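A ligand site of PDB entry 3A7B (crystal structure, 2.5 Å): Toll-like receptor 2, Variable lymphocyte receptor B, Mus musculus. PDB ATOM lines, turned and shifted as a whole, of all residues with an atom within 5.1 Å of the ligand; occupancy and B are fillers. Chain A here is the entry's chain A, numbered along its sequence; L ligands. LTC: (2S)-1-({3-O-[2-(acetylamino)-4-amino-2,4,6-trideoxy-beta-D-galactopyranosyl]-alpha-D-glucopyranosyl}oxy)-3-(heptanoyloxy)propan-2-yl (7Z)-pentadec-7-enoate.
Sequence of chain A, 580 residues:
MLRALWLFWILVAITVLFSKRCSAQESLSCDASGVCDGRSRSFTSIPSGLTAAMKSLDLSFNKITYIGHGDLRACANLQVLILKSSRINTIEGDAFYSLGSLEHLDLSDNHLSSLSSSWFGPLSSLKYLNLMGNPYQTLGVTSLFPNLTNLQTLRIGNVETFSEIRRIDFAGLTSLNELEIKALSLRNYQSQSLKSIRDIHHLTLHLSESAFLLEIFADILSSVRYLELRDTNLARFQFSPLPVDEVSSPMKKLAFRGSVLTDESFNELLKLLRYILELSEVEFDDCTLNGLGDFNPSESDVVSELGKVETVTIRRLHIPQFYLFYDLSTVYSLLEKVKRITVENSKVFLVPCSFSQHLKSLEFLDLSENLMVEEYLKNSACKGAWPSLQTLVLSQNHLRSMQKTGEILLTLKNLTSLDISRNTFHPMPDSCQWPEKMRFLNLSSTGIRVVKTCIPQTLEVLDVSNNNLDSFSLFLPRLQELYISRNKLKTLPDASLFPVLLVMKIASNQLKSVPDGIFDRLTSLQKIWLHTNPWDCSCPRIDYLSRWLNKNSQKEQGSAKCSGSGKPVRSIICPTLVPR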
ATOM      1  N   PHE A 266      21.300  -7.206  10.131  1.00  0.00           N
ATOM      2  CA  PHE A 266      22.520  -7.605   9.460  1.00  0.00           C
ATOM      3  C   PHE A 266      23.115  -6.423   8.683  1.00  0.00           C
ATOM      4  O   PHE A 266      24.333  -6.167   8.709  1.00  0.00           O
ATOM      5  CB  PHE A 266      22.254  -8.772   8.512  1.00  0.00           C
ATOM      6  CG  PHE A 266      23.501  -9.413   7.997  1.00  0.00           C
ATOM      7  CD1 PHE A 266      24.167 -10.375   8.742  1.00  0.00           C
ATOM      8  CD2 PHE A 266      24.066  -9.007   6.801  1.00  0.00           C
ATOM      9  CE1 PHE A 266      25.373 -10.920   8.303  1.00  0.00           C
ATOM     10  CE2 PHE A 266      25.259  -9.538   6.349  1.00  0.00           C
ATOM     11  CZ  PHE A 266      25.918 -10.492   7.102  1.00  0.00           C
ATOM     12  N   LEU A 270      26.694  -4.384   8.908  1.00  0.00           N
ATOM     13  CA  LEU A 270      27.660  -4.228   7.833  1.00  0.00           C
ATOM     14  C   LEU A 270      28.267  -2.853   7.747  1.00  0.00           C
ATOM     15  O   LEU A 270      29.393  -2.707   7.267  1.00  0.00           O
ATOM     16  CB  LEU A 270      27.065  -4.643   6.499  1.00  0.00           C
ATOM     17  CG  LEU A 270      26.888  -6.155   6.371  1.00  0.00           C
ATOM     18  CD1 LEU A 270      26.355  -6.482   4.993  1.00  0.00           C
ATOM     19  CD2 LEU A 270      28.203  -6.837   6.605  1.00  0.00           C
ATOM     20  N   LEU A 306      32.147  -5.250   1.301  1.00  0.00           N
ATOM     21  CA  LEU A 306      32.893  -6.187   2.103  1.00  0.00           C
ATOM     22  C   LEU A 306      34.341  -5.742   2.085  1.00  0.00           C
ATOM     23  O   LEU A 306      35.238  -6.398   2.636  1.00  0.00           O
ATOM     24  CB  LEU A 306      32.759  -7.626   1.599  1.00  0.00           C
ATOM     25  CG  LEU A 306      31.384  -8.179   1.939  1.00  0.00           C
ATOM     26  CD1 LEU A 306      31.367  -9.694   1.749  1.00  0.00           C
ATOM     27  CD2 LEU A 306      31.055  -7.826   3.386  1.00  0.00           C
ATOM     28  N   VAL A 312      34.718 -15.714   3.604  1.00  0.00           N
ATOM     29  CA  VAL A 312      33.463 -15.639   4.341  1.00  0.00           C
ATOM     30  C   VAL A 312      33.230 -17.064   4.811  1.00  0.00           C
ATOM     31  O   VAL A 312      33.183 -17.973   3.997  1.00  0.00           O
ATOM     32  CB  VAL A 312      32.316 -15.266   3.455  1.00  0.00           C
ATOM     33  CG1 VAL A 312      31.027 -15.441   4.225  1.00  0.00           C
ATOM     34  CG2 VAL A 312      32.440 -13.816   2.994  1.00  0.00           C
ATOM     35  N   ILE A 314      30.675 -19.543   6.916  1.00  0.00           N
ATOM     36  CA  ILE A 314      29.414 -19.849   7.610  1.00  0.00           C
ATOM     37  C   ILE A 314      29.261 -21.330   7.966  1.00  0.00           C
ATOM     38  O   ILE A 314      29.480 -22.209   7.122  1.00  0.00           O
ATOM     39  CB  ILE A 314      28.209 -19.456   6.773  1.00  0.00           C
ATOM     40  CG1 ILE A 314      28.339 -17.981   6.454  1.00  0.00           C
ATOM     41  CG2 ILE A 314      26.894 -19.745   7.537  1.00  0.00           C
ATOM     42  CD1 ILE A 314      27.774 -17.637   5.151  1.00  0.00           C
ATOM     43  N   LEU A 317      24.109 -22.412   9.862  1.00  0.00           N
ATOM     44  CA  LEU A 317      23.230 -21.251   9.820  1.00  0.00           C
ATOM     45  C   LEU A 317      21.794 -21.775   9.803  1.00  0.00           C
ATOM     46  O   LEU A 317      21.515 -22.813   9.215  1.00  0.00           O
ATOM     47  CB  LEU A 317      23.510 -20.429   8.559  1.00  0.00           C
ATOM     48  CG  LEU A 317      22.592 -19.220   8.283  1.00  0.00           C
ATOM     49  CD1 LEU A 317      22.764 -18.198   9.388  1.00  0.00           C
ATOM     50  CD2 LEU A 317      22.923 -18.589   6.899  1.00  0.00           C
ATOM     51  N   ILE A 319      18.056 -20.498   8.732  1.00  0.00           N
ATOM     52  CA  ILE A 319      17.136 -19.518   8.175  1.00  0.00           C
ATOM     53  C   ILE A 319      15.751 -20.104   8.405  1.00  0.00           C
ATOM     54  O   ILE A 319      15.581 -21.307   8.279  1.00  0.00           O
ATOM     55  CB  ILE A 319      17.329 -19.351   6.668  1.00  0.00           C
ATOM     56  CG1 ILE A 319      18.611 -18.605   6.358  1.00  0.00           C
ATOM     57  CG2 ILE A 319      16.131 -18.634   6.082  1.00  0.00           C
ATOM     58  CD1 ILE A 319      19.806 -19.435   6.550  1.00  0.00           C
ATOM     59  N   PRO A 320      14.750 -19.279   8.770  1.00  0.00           N
ATOM     60  CA  PRO A 320      13.428 -19.890   8.973  1.00  0.00           C
ATOM     61  C   PRO A 320      12.950 -20.622   7.688  1.00  0.00           C
ATOM     62  O   PRO A 320      13.064 -21.858   7.598  1.00  0.00           O
ATOM     63  CB  PRO A 320      12.531 -18.695   9.321  1.00  0.00           C
ATOM     64  CG  PRO A 320      13.284 -17.488   8.715  1.00  0.00           C
ATOM     65  CD  PRO A 320      14.715 -17.825   9.035  1.00  0.00           C
ATOM     66  N   GLN A 321      12.426 -19.886   6.705  1.00  0.00           N
ATOM     67  CA  GLN A 321      11.961 -20.478   5.447  1.00  0.00           C
ATOM     68  C   GLN A 321      11.970 -19.491   4.260  1.00  0.00           C
ATOM     69  O   GLN A 321      11.414 -18.392   4.351  1.00  0.00           O
ATOM     70  CB  GLN A 321      10.518 -21.058   5.602  1.00  0.00           C
ATOM     71  CG  GLN A 321      10.317 -22.356   6.488  1.00  0.00           C
ATOM     72  CD  GLN A 321      10.219 -23.718   5.697  1.00  0.00           C
ATOM     73  OE1 GLN A 321      10.081 -24.797   6.296  1.00  0.00           O
ATOM     74  NE2 GLN A 321      10.285 -23.647   4.363  1.00  0.00           N
ATOM     75  N   PHE A 322      12.614 -19.875   3.158  1.00  0.00           N
ATOM     76  CA  PHE A 322      12.618 -19.049   1.952  1.00  0.00           C
ATOM     77  C   PHE A 322      11.312 -19.440   1.276  1.00  0.00           C
ATOM     78  O   PHE A 322      11.107 -20.613   0.941  1.00  0.00           O
ATOM     79  CB  PHE A 322      13.755 -19.418   1.003  1.00  0.00           C
ATOM     80  CG  PHE A 322      15.077 -18.802   1.367  1.00  0.00           C
ATOM     81  CD1 PHE A 322      15.834 -19.307   2.424  1.00  0.00           C
ATOM     82  CD2 PHE A 322      15.587 -17.754   0.603  1.00  0.00           C
ATOM     83  CE1 PHE A 322      17.078 -18.769   2.717  1.00  0.00           C
ATOM     84  CE2 PHE A 322      16.829 -17.204   0.880  1.00  0.00           C
ATOM     85  CZ  PHE A 322      17.586 -17.715   1.945  1.00  0.00           C
ATOM     86  N   TYR A 323      10.404 -18.483   1.088  1.00  0.00           N
ATOM     87  CA  TYR A 323       9.112 -18.759   0.457  1.00  0.00           C
ATOM     88  C   TYR A 323       8.840 -17.817  -0.710  1.00  0.00           C
ATOM     89  O   TYR A 323       8.295 -18.227  -1.747  1.00  0.00           O
ATOM     90  CB  TYR A 323       7.999 -18.641   1.506  1.00  0.00           C
ATOM     91  CG  TYR A 323       7.823 -19.871   2.375  1.00  0.00           C
ATOM     92  CD1 TYR A 323       7.282 -19.759   3.662  1.00  0.00           C
ATOM     93  CD2 TYR A 323       8.160 -21.150   1.895  1.00  0.00           C
ATOM     94  CE1 TYR A 323       7.082 -20.885   4.462  1.00  0.00           C
ATOM     95  CE2 TYR A 323       7.974 -22.288   2.671  1.00  0.00           C
ATOM     96  CZ  TYR A 323       7.435 -22.148   3.953  1.00  0.00           C
ATOM     97  OH  TYR A 323       7.249 -23.266   4.719  1.00  0.00           O
ATOM     98  N   LEU A 328      18.969 -10.762  -3.757  1.00  0.00           N
ATOM     99  CA  LEU A 328      20.388 -11.064  -3.860  1.00  0.00           C
ATOM    100  C   LEU A 328      21.202 -10.063  -4.665  1.00  0.00           C
ATOM    101  O   LEU A 328      22.408 -10.219  -4.779  1.00  0.00           O
ATOM    102  CB  LEU A 328      20.583 -12.457  -4.441  1.00  0.00           C
ATOM    103  CG  LEU A 328      19.852 -13.658  -3.833  1.00  0.00           C
ATOM    104  CD1 LEU A 328      20.150 -14.917  -4.667  1.00  0.00           C
ATOM    105  CD2 LEU A 328      20.264 -13.843  -2.390  1.00  0.00           C
ATOM    106  N   VAL A 331      23.536  -8.983  -2.239  1.00  0.00           N
ATOM    107  CA  VAL A 331      24.483 -10.043  -1.920  1.00  0.00           C
ATOM    108  C   VAL A 331      25.460 -10.273  -3.094  1.00  0.00           C
ATOM    109  O   VAL A 331      26.661 -10.482  -2.896  1.00  0.00           O
ATOM    110  CB  VAL A 331      23.767 -11.364  -1.578  1.00  0.00           C
ATOM    111  CG1 VAL A 331      24.785 -12.486  -1.452  1.00  0.00           C
ATOM    112  CG2 VAL A 331      23.003 -11.232  -0.282  1.00  0.00           C
ATOM    113  N   LEU A 334      27.852  -7.583  -2.717  1.00  0.00           N
ATOM    114  CA  LEU A 334      28.590  -7.851  -1.470  1.00  0.00           C
ATOM    115  C   LEU A 334      29.610  -8.993  -1.585  1.00  0.00           C
ATOM    116  O   LEU A 334      30.679  -8.942  -0.988  1.00  0.00           O
ATOM    117  CB  LEU A 334      27.600  -8.225  -0.377  1.00  0.00           C
ATOM    118  CG  LEU A 334      27.481  -7.478   0.955  1.00  0.00           C
ATOM    119  CD1 LEU A 334      27.927  -6.014   0.845  1.00  0.00           C
ATOM    120  CD2 LEU A 334      26.005  -7.615   1.442  1.00  0.00           C
ATOM    121  N   LEU A 335      29.279 -10.029  -2.351  1.00  0.00           N
ATOM    122  CA  LEU A 335      30.179 -11.153  -2.460  1.00  0.00           C
ATOM    123  C   LEU A 335      31.041 -11.104  -3.699  1.00  0.00           C
ATOM    124  O   LEU A 335      31.848 -11.990  -3.932  1.00  0.00           O
ATOM    125  CB  LEU A 335      29.395 -12.463  -2.413  1.00  0.00           C
ATOM    126  CG  LEU A 335      28.736 -12.748  -1.064  1.00  0.00           C
ATOM    127  CD1 LEU A 335      27.994 -14.068  -1.143  1.00  0.00           C
ATOM    128  CD2 LEU A 335      29.780 -12.812   0.014  1.00  0.00           C
ATOM    129  N   VAL A 343      30.039 -22.746   3.380  1.00  0.00           N
ATOM    130  CA  VAL A 343      28.713 -22.725   3.974  1.00  0.00           C
ATOM    131  C   VAL A 343      28.570 -24.147   4.384  1.00  0.00           C
ATOM    132  O   VAL A 343      28.104 -24.987   3.644  1.00  0.00           O
ATOM    133  CB  VAL A 343      27.612 -22.374   3.028  1.00  0.00           C
ATOM    134  CG1 VAL A 343      26.322 -22.477   3.802  1.00  0.00           C
ATOM    135  CG2 VAL A 343      27.784 -20.963   2.531  1.00  0.00           C
ATOM    136  N   SER A 346      24.518 -26.491   6.917  1.00  0.00           N
ATOM    137  CA  SER A 346      23.409 -25.570   7.081  1.00  0.00           C
ATOM    138  C   SER A 346      22.240 -25.992   6.213  1.00  0.00           C
ATOM    139  O   SER A 346      21.493 -25.145   5.757  1.00  0.00           O
ATOM    140  CB  SER A 346      23.808 -24.143   6.701  1.00  0.00           C
ATOM    141  OG  SER A 346      25.001 -23.756   7.340  1.00  0.00           O
ATOM    142  N   LYS A 347      22.108 -27.302   5.953  1.00  0.00           N
ATOM    143  CA  LYS A 347      20.993 -27.818   5.144  1.00  0.00           C
ATOM    144  C   LYS A 347      20.802 -27.151   3.763  1.00  0.00           C
ATOM    145  O   LYS A 347      19.676 -26.915   3.298  1.00  0.00           O
ATOM    146  CB  LYS A 347      19.687 -27.698   5.947  1.00  0.00           C
ATOM    147  CG  LYS A 347      19.787 -28.404   7.314  1.00  0.00           C
ATOM    148  CD  LYS A 347      18.524 -28.233   8.097  1.00  0.00           C
ATOM    149  CE  LYS A 347      18.503 -29.141   9.320  1.00  0.00           C
ATOM    150  NZ  LYS A 347      17.116 -29.161   9.943  1.00  0.00           N
ATOM    151  N   VAL A 348      21.915 -26.849   3.099  1.00  0.00           N
ATOM    152  CA  VAL A 348      21.848 -26.250   1.800  1.00  0.00           C
ATOM    153  C   VAL A 348      21.511 -27.344   0.777  1.00  0.00           C
ATOM    154  O   VAL A 348      22.075 -28.458   0.775  1.00  0.00           O
ATOM    155  CB  VAL A 348      23.193 -25.615   1.461  1.00  0.00           C
ATOM    156  CG1 VAL A 348      23.204 -25.085   0.049  1.00  0.00           C
ATOM    157  CG2 VAL A 348      23.506 -24.514   2.466  1.00  0.00           C
ATOM    158  N   PHE A 349      20.554 -27.044  -0.101  1.00  0.00           N
ATOM    159  CA  PHE A 349      20.192 -28.006  -1.123  1.00  0.00           C
ATOM    160  C   PHE A 349      20.313 -27.302  -2.472  1.00  0.00           C
ATOM    161  O   PHE A 349      20.224 -27.919  -3.528  1.00  0.00           O
ATOM    162  CB  PHE A 349      18.769 -28.521  -0.872  1.00  0.00           C
ATOM    163  CG  PHE A 349      17.701 -27.521  -1.144  1.00  0.00           C
ATOM    164  CD1 PHE A 349      17.359 -27.177  -2.467  1.00  0.00           C
ATOM    165  CD2 PHE A 349      17.011 -26.912  -0.094  1.00  0.00           C
ATOM    166  CE1 PHE A 349      16.386 -26.243  -2.738  1.00  0.00           C
ATOM    167  CE2 PHE A 349      16.014 -25.979  -0.337  1.00  0.00           C
ATOM    168  CZ  PHE A 349      15.701 -25.638  -1.667  1.00  0.00           C
ATOM    169  N   LEU A 350      20.544 -25.998  -2.444  1.00  0.00           N
ATOM    170  CA  LEU A 350      20.674 -25.255  -3.691  1.00  0.00           C
ATOM    171  C   LEU A 350      21.384 -23.906  -3.586  1.00  0.00           C
ATOM    172  O   LEU A 350      21.316 -23.226  -2.573  1.00  0.00           O
ATOM    173  CB  LEU A 350      19.275 -25.021  -4.255  1.00  0.00           C
ATOM    174  CG  LEU A 350      19.155 -24.040  -5.415  1.00  0.00           C
ATOM    175  CD1 LEU A 350      19.703 -24.724  -6.675  1.00  0.00           C
ATOM    176  CD2 LEU A 350      17.717 -23.632  -5.583  1.00  0.00           C
ATOM    177  N   PRO A 352      21.342 -20.953  -6.243  1.00  0.00           N
ATOM    178  CA  PRO A 352      20.842 -20.605  -7.578  1.00  0.00           C
ATOM    179  C   PRO A 352      21.903 -20.236  -8.585  1.00  0.00           C
ATOM    180  O   PRO A 352      22.900 -19.572  -8.263  1.00  0.00           O
ATOM    181  CB  PRO A 352      19.909 -19.432  -7.328  1.00  0.00           C
ATOM    182  CG  PRO A 352      19.538 -19.581  -5.845  1.00  0.00           C
ATOM    183  CD  PRO A 352      20.840 -20.007  -5.234  1.00  0.00           C
ATOM    184  N   PHE A 355      23.072 -16.722  -8.649  1.00  0.00           N
ATOM    185  CA  PHE A 355      23.997 -16.416  -7.568  1.00  0.00           C
ATOM    186  C   PHE A 355      25.393 -16.859  -7.997  1.00  0.00           C
ATOM    187  O   PHE A 355      26.318 -16.074  -8.088  1.00  0.00           O
ATOM    188  CB  PHE A 355      23.548 -17.154  -6.321  1.00  0.00           C
ATOM    189  CG  PHE A 355      24.115 -16.603  -5.045  1.00  0.00           C
ATOM    190  CD1 PHE A 355      25.419 -16.113  -4.997  1.00  0.00           C
ATOM    191  CD2 PHE A 355      23.382 -16.640  -3.878  1.00  0.00           C
ATOM    192  CE1 PHE A 355      25.978 -15.674  -3.827  1.00  0.00           C
ATOM    193  CE2 PHE A 355      23.921 -16.212  -2.702  1.00  0.00           C
ATOM    194  CZ  PHE A 355      25.233 -15.731  -2.661  1.00  0.00           C
ATOM    195  N   LEU A 371      22.860 -30.869   1.735  1.00  0.00           N
ATOM    196  CA  LEU A 371      21.895 -31.750   1.098  1.00  0.00           C
ATOM    197  C   LEU A 371      21.944 -31.671  -0.402  1.00  0.00           C
ATOM    198  O   LEU A 371      20.919 -31.738  -1.067  1.00  0.00           O
ATOM    199  CB  LEU A 371      20.478 -31.391   1.568  1.00  0.00           C
ATOM    200  CG  LEU A 371      19.927 -31.880   2.913  1.00  0.00           C
ATOM    201  CD1 LEU A 371      20.973 -32.422   3.814  1.00  0.00           C
ATOM    202  CD2 LEU A 371      19.240 -30.724   3.553  1.00  0.00           C
HETATM  203  C1  LTC L   1      12.604 -24.927   2.107  1.00  0.00           C
HETATM  204  O1  LTC L   1      12.596 -23.725   2.884  1.00  0.00           O
HETATM  205  C2  LTC L   1      11.999 -26.068   2.954  1.00  0.00           C
HETATM  206  O2  LTC L   1      12.175 -27.201   5.083  1.00  0.00           O
HETATM  207  C3  LTC L   1      12.840 -26.271   4.209  1.00  0.00           C
HETATM  208  O3  LTC L   1      14.042 -25.113   5.967  1.00  0.00           O
HETATM  209  C4  LTC L   1      13.064 -24.938   4.936  1.00  0.00           C
HETATM  210  O4  LTC L   1      11.978 -27.267   2.185  1.00  0.00           O
HETATM  211  C5  LTC L   1      13.537 -23.853   3.954  1.00  0.00           C
HETATM  212  O5  LTC L   1      12.430 -23.720   0.033  1.00  0.00           O
HETATM  213  C7  LTC L   1      11.803 -24.748   0.816  1.00  0.00           C
HETATM  214  O9  LTC L   1      19.464 -24.270   2.754  1.00  0.00           O
HETATM  215  O10 LTC L   1      18.108 -22.634   3.469  1.00  0.00           O
HETATM  216  C11 LTC L   1      28.805 -11.296   3.189  1.00  0.00           C
HETATM  217  O11 LTC L   1      14.790 -24.214   3.357  1.00  0.00           O
HETATM  218  C12 LTC L   1      27.324 -11.225   3.542  1.00  0.00           C
HETATM  219  O12 LTC L   1      18.032 -22.809   0.873  1.00  0.00           O
HETATM  220  C13 LTC L   1      26.739 -12.620   3.773  1.00  0.00           C
HETATM  221  O13 LTC L   1      16.625 -22.465  -0.834  1.00  0.00           O
HETATM  222  C14 LTC L   1      26.767 -13.471   2.502  1.00  0.00           C
HETATM  223  C15 LTC L   1      26.228 -14.879   2.805  1.00  0.00           C
HETATM  224  C16 LTC L   1      26.143 -15.741   1.542  1.00  0.00           C
HETATM  225  C17 LTC L   1      25.590 -17.123   1.904  1.00  0.00           C
HETATM  226  C18 LTC L   1      25.285 -17.962   0.665  1.00  0.00           C
HETATM  227  C19 LTC L   1      24.589 -19.278   1.045  1.00  0.00           C
HETATM  228  C20 LTC L   1      23.485 -19.029   2.064  1.00  0.00           C
HETATM  229  C21 LTC L   1      22.612 -20.261   2.306  1.00  0.00           C
HETATM  230  C22 LTC L   1      21.572 -19.954   3.396  1.00  0.00           C
HETATM  231  C23 LTC L   1      20.325 -20.831   3.267  1.00  0.00           C
HETATM  232  C24 LTC L   1      20.592 -22.315   3.559  1.00  0.00           C
HETATM  233  C25 LTC L   1      19.353 -23.135   3.220  1.00  0.00           C
HETATM  234  C26 LTC L   1      17.106 -23.561   3.004  1.00  0.00           C
HETATM  235  C27 LTC L   1      15.831 -23.325   3.788  1.00  0.00           C
HETATM  236  C28 LTC L   1      16.852 -23.281   1.521  1.00  0.00           C
HETATM  237  C29 LTC L   1      17.735 -22.312  -0.381  1.00  0.00           C
HETATM  238  C30 LTC L   1      18.811 -21.575  -1.168  1.00  0.00           C
HETATM  239  C31 LTC L   1      18.854 -20.127  -0.657  1.00  0.00           C
HETATM  240  C32 LTC L   1      20.042 -19.317  -1.181  1.00  0.00           C
HETATM  241  C33 LTC L   1      20.065 -17.978  -0.434  1.00  0.00           C
HETATM  242  C34 LTC L   1      21.281 -17.111  -0.782  1.00  0.00           C
HETATM  243  C35 LTC L   1      21.281 -15.844   0.078  1.00  0.00           C
HETATM  244  C41 LTC L   1      14.907 -29.479   5.760  1.00  0.00           C
HETATM  245  O41 LTC L   1      13.908 -28.770   5.014  1.00  0.00           O
HETATM  246  C42 LTC L   1      14.227 -30.455   6.726  1.00  0.00           C
HETATM  247  N42 LTC L   1      13.438 -31.418   5.955  1.00  0.00           N
HETATM  248  O42 LTC L   1      12.585 -30.602   8.482  1.00  0.00           O
HETATM  249  C43 LTC L   1      13.327 -29.681   7.679  1.00  0.00           C
HETATM  250  C44 LTC L   1      12.358 -28.810   6.885  1.00  0.00           C
HETATM  251  N44 LTC L   1      11.572 -27.965   7.797  1.00  0.00           N
HETATM  252  C45 LTC L   1      13.118 -27.934   5.870  1.00  0.00           C
HETATM  253  C47 LTC L   1      15.803 -30.256   4.795  1.00  0.00           C
HETATM  254  C48 LTC L   1      10.333 -28.261   8.145  1.00  0.00           C
HETATM  255  O48 LTC L   1       9.649 -27.572   8.915  1.00  0.00           O
HETATM  256  C49 LTC L   1       9.772 -29.545   7.541  1.00  0.00           C
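The backbone carbonyl oxygen (O) of Lys 347 lies close to an oxygen (O9) of the ligand (2.7 Å).
The backbone carbonyl oxygen (O) of Phe 322 lies within hydrogen-bond range of an oxygen (O5) of the ligand (3.5 Å).
NE2 of Gln 321 is in hydrogen-bond range of O1 of the ligand (2.7 Å).
The backbone NH of Leu 317 sits at hydrogen-bond distance from the side-chain hydroxyl of Ser 346, 3.0 Å away.
N of Leu 371 lies within hydrogen-bond range of O of Val 348 (2.7 Å).
The side-chain hydroxyl (OH) of Tyr 323 sits at hydrogen-bond distance from the side-chain amide nitrogen (NE2) of Gln 321 (3.1 Å).
Phe 266 touches the ligand.
Leu 306 touches the ligand (CD1 to C11, 3.3 Å).
CD1 of Ile 314 touches C15 of the ligand, at 3.9 Å.
Leu 317 touches the ligand (CD2 to C22, 3.99 Å).
Ile 319 touches the ligand.
O of Pro 320 touches O3 of the ligand, at 3.8 Å.
Leu 328 touches the ligand.
CD2 of Leu 335 touches C11 of the ligand, at 3.7 Å.
Val 343 touches the ligand (CG2 to C19, 3.9 Å).
Ser 346 touches the ligand (O to C24, 3.7 Å).
Val 348 touches the ligand.
CE2 of Phe 349 touches C28 of the ligand (3.4 Å).
Leu 350 touches the ligand.
Phe 355 touches the ligand (CE2 to C34, 3.4 Å).
CD2 of Leu 371 touches C47 of the ligand (3.7 Å).
Hydrophobic or aromatic side chains that line the ligand: Phe 266, Leu 306, Ile 314, Leu 317, Ile 319, Phe 322, Leu 328, Leu 335, Val 343, Val 348, Phe 349, Phe 355 and Leu 371.
Along chain A the residues within 4 Å of the ligand span positions 266 to 371.
The nearest printed residue that does not touch the ligand is Pro 352 (4.2 Å).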
